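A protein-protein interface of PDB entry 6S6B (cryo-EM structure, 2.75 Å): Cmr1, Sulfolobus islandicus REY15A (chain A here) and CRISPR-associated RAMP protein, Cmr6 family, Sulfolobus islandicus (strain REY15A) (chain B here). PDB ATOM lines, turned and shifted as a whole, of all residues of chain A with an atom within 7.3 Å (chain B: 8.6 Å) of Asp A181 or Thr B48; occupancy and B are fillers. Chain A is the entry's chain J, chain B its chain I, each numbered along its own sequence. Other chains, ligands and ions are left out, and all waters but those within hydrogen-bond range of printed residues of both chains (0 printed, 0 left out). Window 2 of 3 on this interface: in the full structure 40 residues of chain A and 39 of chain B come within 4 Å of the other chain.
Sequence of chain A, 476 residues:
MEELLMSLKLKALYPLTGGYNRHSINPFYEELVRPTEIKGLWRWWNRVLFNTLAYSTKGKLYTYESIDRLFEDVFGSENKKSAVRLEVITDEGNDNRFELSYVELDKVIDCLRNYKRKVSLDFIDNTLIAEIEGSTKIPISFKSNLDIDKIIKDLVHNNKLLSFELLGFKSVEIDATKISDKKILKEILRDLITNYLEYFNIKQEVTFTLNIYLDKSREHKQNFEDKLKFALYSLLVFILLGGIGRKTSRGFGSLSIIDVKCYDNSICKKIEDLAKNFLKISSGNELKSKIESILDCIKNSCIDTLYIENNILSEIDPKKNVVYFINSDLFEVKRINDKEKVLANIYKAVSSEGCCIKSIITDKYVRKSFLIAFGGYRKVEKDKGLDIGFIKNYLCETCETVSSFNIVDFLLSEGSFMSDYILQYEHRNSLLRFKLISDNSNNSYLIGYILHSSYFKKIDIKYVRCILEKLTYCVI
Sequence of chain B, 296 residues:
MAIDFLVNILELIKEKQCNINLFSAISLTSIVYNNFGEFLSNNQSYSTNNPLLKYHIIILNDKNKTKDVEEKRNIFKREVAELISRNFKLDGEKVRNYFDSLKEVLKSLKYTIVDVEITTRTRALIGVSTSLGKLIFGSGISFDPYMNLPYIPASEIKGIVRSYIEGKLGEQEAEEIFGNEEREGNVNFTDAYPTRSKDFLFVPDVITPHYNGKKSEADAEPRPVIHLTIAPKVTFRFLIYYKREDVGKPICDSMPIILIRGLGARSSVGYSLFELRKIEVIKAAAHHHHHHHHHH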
ATOM      1  N   ILE A 109     -23.743  26.246   8.616  1.00  0.00           N
ATOM      2  CA  ILE A 109     -24.822  26.683   9.493  1.00  0.00           C
ATOM      3  C   ILE A 109     -26.079  26.939   8.678  1.00  0.00           C
ATOM      4  O   ILE A 109     -27.154  26.400   8.963  1.00  0.00           O
ATOM      5  CB  ILE A 109     -24.400  27.935  10.279  1.00  0.00           C
ATOM      6  CG1 ILE A 109     -23.286  27.597  11.265  1.00  0.00           C
ATOM      7  CG2 ILE A 109     -25.593  28.527  11.001  1.00  0.00           C
ATOM      8  CD1 ILE A 109     -22.942  28.734  12.189  1.00  0.00           C
ATOM      9  N   LEU A 112     -28.072  24.127   7.440  1.00  0.00           N
ATOM     10  CA  LEU A 112     -28.614  23.269   8.487  1.00  0.00           C
ATOM     11  C   LEU A 112     -29.841  23.860   9.166  1.00  0.00           C
ATOM     12  O   LEU A 112     -30.113  23.529  10.322  1.00  0.00           O
ATOM     13  CB  LEU A 112     -27.547  22.981   9.540  1.00  0.00           C
ATOM     14  CG  LEU A 112     -26.611  21.805   9.303  1.00  0.00           C
ATOM     15  CD1 LEU A 112     -25.510  21.837  10.336  1.00  0.00           C
ATOM     16  CD2 LEU A 112     -27.377  20.502   9.377  1.00  0.00           C
ATOM     17  N   ARG A 113     -30.584  24.726   8.493  1.00  0.00           N
ATOM     18  CA  ARG A 113     -31.788  25.280   9.089  1.00  0.00           C
ATOM     19  C   ARG A 113     -32.992  24.418   8.744  1.00  0.00           C
ATOM     20  O   ARG A 113     -33.083  23.849   7.653  1.00  0.00           O
ATOM     21  CB  ARG A 113     -32.018  26.713   8.616  1.00  0.00           C
ATOM     22  CG  ARG A 113     -30.740  27.499   8.397  1.00  0.00           C
ATOM     23  CD  ARG A 113     -30.269  28.160   9.681  1.00  0.00           C
ATOM     24  NE  ARG A 113     -29.230  29.152   9.427  1.00  0.00           N
ATOM     25  CZ  ARG A 113     -29.444  30.330   8.849  1.00  0.00           C
ATOM     26  NH1 ARG A 113     -28.437  31.170   8.658  1.00  0.00           N
ATOM     27  NH2 ARG A 113     -30.667  30.679   8.477  1.00  0.00           N
ATOM     28  N   ALA A 176     -33.020  20.692  13.780  1.00  0.00           N
ATOM     29  CA  ALA A 176     -33.297  22.100  13.551  1.00  0.00           C
ATOM     30  C   ALA A 176     -34.705  22.376  13.050  1.00  0.00           C
ATOM     31  O   ALA A 176     -35.013  23.533  12.752  1.00  0.00           O
ATOM     32  CB  ALA A 176     -32.282  22.693  12.562  1.00  0.00           C
ATOM     33  N   LYS A 178     -37.343  22.382  14.836  1.00  0.00           N
ATOM     34  CA  LYS A 178     -37.852  23.273  15.867  1.00  0.00           C
ATOM     35  C   LYS A 178     -37.001  24.540  15.898  1.00  0.00           C
ATOM     36  O   LYS A 178     -36.236  24.826  14.972  1.00  0.00           O
ATOM     37  CB  LYS A 178     -37.883  22.558  17.211  1.00  0.00           C
ATOM     38  CG  LYS A 178     -39.097  21.673  17.409  1.00  0.00           C
ATOM     39  CD  LYS A 178     -40.368  22.502  17.462  1.00  0.00           C
ATOM     40  CE  LYS A 178     -40.295  23.558  18.549  1.00  0.00           C
ATOM     41  NZ  LYS A 178     -41.253  24.670  18.297  1.00  0.00           N
ATOM     42  N   ILE A 179     -37.152  25.332  16.963  1.00  0.00           N
ATOM     43  CA  ILE A 179     -36.393  26.569  17.099  1.00  0.00           C
ATOM     44  C   ILE A 179     -34.899  26.300  16.978  1.00  0.00           C
ATOM     45  O   ILE A 179     -34.354  25.379  17.595  1.00  0.00           O
ATOM     46  CB  ILE A 179     -36.734  27.261  18.432  1.00  0.00           C
ATOM     47  CG1 ILE A 179     -35.973  28.585  18.561  1.00  0.00           C
ATOM     48  CG2 ILE A 179     -36.480  26.333  19.614  1.00  0.00           C
ATOM     49  CD1 ILE A 179     -36.458  29.467  19.689  1.00  0.00           C
ATOM     50  N   SER A 180     -34.235  27.116  16.163  1.00  0.00           N
ATOM     51  CA  SER A 180     -32.806  27.003  15.934  1.00  0.00           C
ATOM     52  C   SER A 180     -32.153  28.356  16.168  1.00  0.00           C
ATOM     53  O   SER A 180     -32.816  29.340  16.504  1.00  0.00           O
ATOM     54  CB  SER A 180     -32.497  26.507  14.519  1.00  0.00           C
ATOM     55  OG  SER A 180     -33.021  25.210  14.319  1.00  0.00           O
ATOM     56  N   ASP A 181     -30.838  28.391  15.987  1.00  0.00           N
ATOM     57  CA  ASP A 181     -30.052  29.598  16.173  1.00  0.00           C
ATOM     58  C   ASP A 181     -28.779  29.468  15.350  1.00  0.00           C
ATOM     59  O   ASP A 181     -28.594  28.507  14.600  1.00  0.00           O
ATOM     60  CB  ASP A 181     -29.741  29.828  17.660  1.00  0.00           C
ATOM     61  CG  ASP A 181     -29.295  31.249  17.960  1.00  0.00           C
ATOM     62  OD1 ASP A 181     -28.424  31.771  17.233  1.00  0.00           O
ATOM     63  OD2 ASP A 181     -29.813  31.844  18.927  1.00  0.00           O
ATOM     64  N   LYS A 182     -27.902  30.456  15.487  1.00  0.00           N
ATOM     65  CA  LYS A 182     -26.559  30.411  14.933  1.00  0.00           C
ATOM     66  C   LYS A 182     -25.505  30.486  16.024  1.00  0.00           C
ATOM     67  O   LYS A 182     -24.554  29.702  16.021  1.00  0.00           O
ATOM     68  CB  LYS A 182     -26.353  31.548  13.924  1.00  0.00           C
ATOM     69  CG  LYS A 182     -27.229  31.452  12.681  1.00  0.00           C
ATOM     70  CD  LYS A 182     -28.614  32.031  12.926  1.00  0.00           C
ATOM     71  CE  LYS A 182     -29.408  32.126  11.648  1.00  0.00           C
ATOM     72  NZ  LYS A 182     -30.810  32.557  11.897  1.00  0.00           N
ATOM     73  N   LYS A 183     -25.669  31.408  16.975  1.00  0.00           N
ATOM     74  CA  LYS A 183     -24.790  31.447  18.138  1.00  0.00           C
ATOM     75  C   LYS A 183     -24.784  30.117  18.876  1.00  0.00           C
ATOM     76  O   LYS A 183     -23.806  29.786  19.554  1.00  0.00           O
ATOM     77  CB  LYS A 183     -25.220  32.575  19.076  1.00  0.00           C
ATOM     78  CG  LYS A 183     -24.216  32.912  20.162  1.00  0.00           C
ATOM     79  CD  LYS A 183     -22.917  33.449  19.583  1.00  0.00           C
ATOM     80  CE  LYS A 183     -21.853  33.581  20.663  1.00  0.00           C
ATOM     81  NZ  LYS A 183     -20.563  34.088  20.124  1.00  0.00           N
ATOM     82  N   ILE A 184     -25.855  29.342  18.755  1.00  0.00           N
ATOM     83  CA  ILE A 184     -25.888  28.006  19.338  1.00  0.00           C
ATOM     84  C   ILE A 184     -25.322  26.974  18.378  1.00  0.00           C
ATOM     85  O   ILE A 184     -24.581  26.078  18.789  1.00  0.00           O
ATOM     86  CB  ILE A 184     -27.324  27.654  19.765  1.00  0.00           C
ATOM     87  CG1 ILE A 184     -27.757  28.556  20.916  1.00  0.00           C
ATOM     88  CG2 ILE A 184     -27.407  26.215  20.196  1.00  0.00           C
ATOM     89  CD1 ILE A 184     -26.831  28.484  22.110  1.00  0.00           C
ATOM     90  N   LEU A 185     -25.643  27.086  17.090  1.00  0.00           N
ATOM     91  CA  LEU A 185     -25.087  26.153  16.121  1.00  0.00           C
ATOM     92  C   LEU A 185     -23.611  26.418  15.871  1.00  0.00           C
ATOM     93  O   LEU A 185     -22.849  25.477  15.632  1.00  0.00           O
ATOM     94  CB  LEU A 185     -25.872  26.224  14.816  1.00  0.00           C
ATOM     95  CG  LEU A 185     -27.247  25.564  14.876  1.00  0.00           C
ATOM     96  CD1 LEU A 185     -27.875  25.507  13.498  1.00  0.00           C
ATOM     97  CD2 LEU A 185     -27.130  24.178  15.474  1.00  0.00           C
ATOM     98  N   LYS A 186     -23.185  27.680  15.925  1.00  0.00           N
ATOM     99  CA  LYS A 186     -21.769  27.976  15.759  1.00  0.00           C
ATOM    100  C   LYS A 186     -20.930  27.419  16.896  1.00  0.00           C
ATOM    101  O   LYS A 186     -19.720  27.256  16.727  1.00  0.00           O
ATOM    102  CB  LYS A 186     -21.544  29.482  15.646  1.00  0.00           C
ATOM    103  CG  LYS A 186     -20.376  29.870  14.763  1.00  0.00           C
ATOM    104  CD  LYS A 186     -19.153  30.217  15.588  1.00  0.00           C
ATOM    105  CE  LYS A 186     -18.042  30.761  14.709  1.00  0.00           C
ATOM    106  NZ  LYS A 186     -16.754  30.887  15.445  1.00  0.00           N
ATOM    107  N   GLU B  11     -24.862  31.333  32.286  1.00  0.00           N
ATOM    108  CA  GLU B  11     -24.433  32.554  31.620  1.00  0.00           C
ATOM    109  C   GLU B  11     -23.686  33.474  32.571  1.00  0.00           C
ATOM    110  O   GLU B  11     -22.803  34.225  32.143  1.00  0.00           O
ATOM    111  CB  GLU B  11     -25.635  33.285  31.036  1.00  0.00           C
ATOM    112  CG  GLU B  11     -26.457  32.473  30.067  1.00  0.00           C
ATOM    113  CD  GLU B  11     -27.704  33.211  29.638  1.00  0.00           C
ATOM    114  OE1 GLU B  11     -28.225  34.014  30.441  1.00  0.00           O
ATOM    115  OE2 GLU B  11     -28.161  33.000  28.497  1.00  0.00           O
ATOM    116  N   LYS B  14     -19.740  32.660  32.603  1.00  0.00           N
ATOM    117  CA  LYS B  14     -18.940  33.077  31.460  1.00  0.00           C
ATOM    118  C   LYS B  14     -18.924  34.582  31.238  1.00  0.00           C
ATOM    119  O   LYS B  14     -18.227  35.042  30.330  1.00  0.00           O
ATOM    120  CB  LYS B  14     -19.435  32.375  30.196  1.00  0.00           C
ATOM    121  CG  LYS B  14     -20.877  32.657  29.855  1.00  0.00           C
ATOM    122  CD  LYS B  14     -21.252  31.987  28.551  1.00  0.00           C
ATOM    123  CE  LYS B  14     -21.245  30.473  28.689  1.00  0.00           C
ATOM    124  NZ  LYS B  14     -22.295  29.970  29.612  1.00  0.00           N
ATOM    125  N   SER B  45     -37.859  30.203  26.928  1.00  0.00           N
ATOM    126  CA  SER B  45     -37.530  31.518  27.479  1.00  0.00           C
ATOM    127  C   SER B  45     -36.050  31.613  27.811  1.00  0.00           C
ATOM    128  O   SER B  45     -35.648  32.359  28.706  1.00  0.00           O
ATOM    129  CB  SER B  45     -38.376  31.872  28.707  1.00  0.00           C
ATOM    130  OG  SER B  45     -38.016  31.069  29.820  1.00  0.00           O
ATOM    131  N   TYR B  46     -35.240  30.853  27.086  1.00  0.00           N
ATOM    132  CA  TYR B  46     -33.798  30.861  27.243  1.00  0.00           C
ATOM    133  C   TYR B  46     -33.194  31.871  26.281  1.00  0.00           C
ATOM    134  O   TYR B  46     -33.641  31.996  25.137  1.00  0.00           O
ATOM    135  CB  TYR B  46     -33.221  29.473  26.977  1.00  0.00           C
ATOM    136  CG  TYR B  46     -33.434  28.475  28.088  1.00  0.00           C
ATOM    137  CD1 TYR B  46     -33.016  27.162  27.948  1.00  0.00           C
ATOM    138  CD2 TYR B  46     -34.051  28.843  29.274  1.00  0.00           C
ATOM    139  CE1 TYR B  46     -33.205  26.245  28.950  1.00  0.00           C
ATOM    140  CE2 TYR B  46     -34.246  27.928  30.285  1.00  0.00           C
ATOM    141  CZ  TYR B  46     -33.819  26.631  30.118  1.00  0.00           C
ATOM    142  OH  TYR B  46     -34.009  25.710  31.121  1.00  0.00           O
ATOM    143  N   SER B  47     -32.178  32.589  26.749  1.00  0.00           N
ATOM    144  CA  SER B  47     -31.559  33.620  25.935  1.00  0.00           C
ATOM    145  C   SER B  47     -30.737  33.000  24.810  1.00  0.00           C
ATOM    146  O   SER B  47     -30.580  31.780  24.706  1.00  0.00           O
ATOM    147  CB  SER B  47     -30.676  34.520  26.797  1.00  0.00           C
ATOM    148  OG  SER B  47     -30.017  35.490  26.001  1.00  0.00           O
ATOM    149  N   THR B  48     -30.219  33.875  23.944  1.00  0.00           N
ATOM    150  CA  THR B  48     -29.271  33.441  22.925  1.00  0.00           C
ATOM    151  C   THR B  48     -27.996  32.913  23.568  1.00  0.00           C
ATOM    152  O   THR B  48     -27.391  31.951  23.080  1.00  0.00           O
ATOM    153  CB  THR B  48     -28.953  34.602  21.983  1.00  0.00           C
ATOM    154  OG1 THR B  48     -30.166  35.094  21.403  1.00  0.00           O
ATOM    155  CG2 THR B  48     -28.020  34.154  20.867  1.00  0.00           C
ATOM    156  N   ASN B  49     -27.578  33.533  24.673  1.00  0.00           N
ATOM    157  CA  ASN B  49     -26.404  33.102  25.415  1.00  0.00           C
ATOM    158  C   ASN B  49     -26.623  31.787  26.143  1.00  0.00           C
ATOM    159  O   ASN B  49     -25.659  31.231  26.677  1.00  0.00           O
ATOM    160  CB  ASN B  49     -26.009  34.177  26.426  1.00  0.00           C
ATOM    161  CG  ASN B  49     -25.357  35.377  25.779  1.00  0.00           C
ATOM    162  OD1 ASN B  49     -25.728  35.781  24.678  1.00  0.00           O
ATOM    163  ND2 ASN B  49     -24.382  35.959  26.465  1.00  0.00           N
ATOM    164  N   ASN B  50     -27.848  31.282  26.172  1.00  0.00           N
ATOM    165  CA  ASN B  50     -28.170  30.153  27.034  1.00  0.00           C
ATOM    166  C   ASN B  50     -27.486  28.886  26.538  1.00  0.00           C
ATOM    167  O   ASN B  50     -27.580  28.557  25.350  1.00  0.00           O
ATOM    168  CB  ASN B  50     -29.673  29.942  27.099  1.00  0.00           C
ATOM    169  CG  ASN B  50     -30.065  28.937  28.146  1.00  0.00           C
ATOM    170  OD1 ASN B  50     -29.899  27.736  27.959  1.00  0.00           O
ATOM    171  ND2 ASN B  50     -30.584  29.421  29.264  1.00  0.00           N
ATOM    172  N   PRO B  51     -26.798  28.152  27.410  1.00  0.00           N
ATOM    173  CA  PRO B  51     -26.114  26.918  27.006  1.00  0.00           C
ATOM    174  C   PRO B  51     -26.941  25.648  27.135  1.00  0.00           C
ATOM    175  O   PRO B  51     -26.367  24.561  27.056  1.00  0.00           O
ATOM    176  CB  PRO B  51     -24.934  26.878  27.981  1.00  0.00           C
ATOM    177  CG  PRO B  51     -25.496  27.481  29.223  1.00  0.00           C
ATOM    178  CD  PRO B  51     -26.503  28.517  28.804  1.00  0.00           C
ATOM    179  N   LEU B  52     -28.253  25.744  27.345  1.00  0.00           N
ATOM    180  CA  LEU B  52     -29.086  24.554  27.396  1.00  0.00           C
ATOM    181  C   LEU B  52     -29.793  24.263  26.082  1.00  0.00           C
ATOM    182  O   LEU B  52     -30.249  23.134  25.884  1.00  0.00           O
ATOM    183  CB  LEU B  52     -30.128  24.671  28.512  1.00  0.00           C
ATOM    184  CG  LEU B  52     -29.728  24.133  29.886  1.00  0.00           C
ATOM    185  CD1 LEU B  52     -30.875  24.274  30.862  1.00  0.00           C
ATOM    186  CD2 LEU B  52     -29.295  22.689  29.786  1.00  0.00           C
ATOM    187  N   LEU B  53     -29.906  25.251  25.190  1.00  0.00           N
ATOM    188  CA  LEU B  53     -30.428  24.977  23.857  1.00  0.00           C
ATOM    189  C   LEU B  53     -29.601  23.912  23.160  1.00  0.00           C
ATOM    190  O   LEU B  53     -30.141  23.078  22.425  1.00  0.00           O
ATOM    191  CB  LEU B  53     -30.441  26.246  23.009  1.00  0.00           C
ATOM    192  CG  LEU B  53     -31.536  27.284  23.200  1.00  0.00           C
ATOM    193  CD1 LEU B  53     -31.275  28.092  24.443  1.00  0.00           C
ATOM    194  CD2 LEU B  53     -31.612  28.175  21.977  1.00  0.00           C
ATOM    195  N   LYS B  54     -28.285  23.942  23.371  1.00  0.00           N
ATOM    196  CA  LYS B  54     -27.382  23.008  22.710  1.00  0.00           C
ATOM    197  C   LYS B  54     -27.858  21.571  22.847  1.00  0.00           C
ATOM    198  O   LYS B  54     -27.774  20.787  21.897  1.00  0.00           O
ATOM    199  CB  LYS B  54     -25.977  23.170  23.284  1.00  0.00           C
ATOM    200  CG  LYS B  54     -24.948  22.256  22.676  1.00  0.00           C
ATOM    201  CD  LYS B  54     -23.693  22.212  23.514  1.00  0.00           C
ATOM    202  CE  LYS B  54     -23.268  23.603  23.937  1.00  0.00           C
ATOM    203  NZ  LYS B  54     -22.190  23.558  24.960  1.00  0.00           N
ATOM    204  N   ILE B  57     -31.022  21.001  20.557  1.00  0.00           N
ATOM    205  CA  ILE B  57     -30.633  20.820  19.161  1.00  0.00           C
ATOM    206  C   ILE B  57     -29.913  19.494  18.977  1.00  0.00           C
ATOM    207  O   ILE B  57     -30.297  18.666  18.146  1.00  0.00           O
ATOM    208  CB  ILE B  57     -29.760  21.997  18.697  1.00  0.00           C
ATOM    209  CG1 ILE B  57     -30.602  23.261  18.566  1.00  0.00           C
ATOM    210  CG2 ILE B  57     -29.084  21.664  17.389  1.00  0.00           C
ATOM    211  CD1 ILE B  57     -29.803  24.478  18.233  1.00  0.00           C
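Among the printed residues, merely in contact across the chains: Asp A181 with Thr B48, Lys A183 with Thr B48, Ile A184 with Thr B48, Ile A184 with Asn B50, Ile A184 with Ile B57 and Leu A185 with Ile B57.
Printed residues of chain B that touch a printed residue of chain A: Thr B48, Asn B50 and Ile B57. Hydrophobic or aromatic side chains of chain B that line the printed part of chain A: Ile B57. Hydrophobic or aromatic side chains of chain A that line the printed part of chain B: Ile A184 and Leu A185. Along chain A the printed residues that touch a printed residue of chain B span positions 181 to 185. Among the printed residues, 6 pairs touch across the chains.
No residue of chain B comes within 4 Å of Ser A180. Of the printed residues of chain B, Ile A184 touches Thr B48 (3.6 Å), Asn B50 (3.3 Å) and Ile B57 (3.6 Å). Printed residues of chain B within 4 Å of Leu A185: Ile B57 (3.7 Å). Glu B11 touches none of the printed residues of chain A. Thr B48 touches just these residues of chain A: Asp A181 (3.5 Å), Lys A183 (3.7 Å) and Ile A184 (3.6 Å). Printed residues of chain A within 4 Å of Asn B50: Ile A184 (3.3 Å). The nearest residue of chain B that does not touch Asp A181 is Ile B57 (4.6 Å). The nearest residue of chain A that does not touch Thr B48 is Lys A182 (6.5 Å). The nearest printed residue of chain B that does not touch Leu A185 is Lys B54 (7.2 Å).
The backbone NH (N) of Asn B50 sits at hydrogen-bond distance from the side-chain carboxylate (OE2) of Glu B11 (2.9 Å). OD1 of Asn B50 sits at hydrogen-bond distance from N of Leu B52 (2.7 Å). The side-chain carboxylate (OD1) of Asp A181 sits at hydrogen-bond distance from the backbone NH (N) of Lys A183 (2.8 Å).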
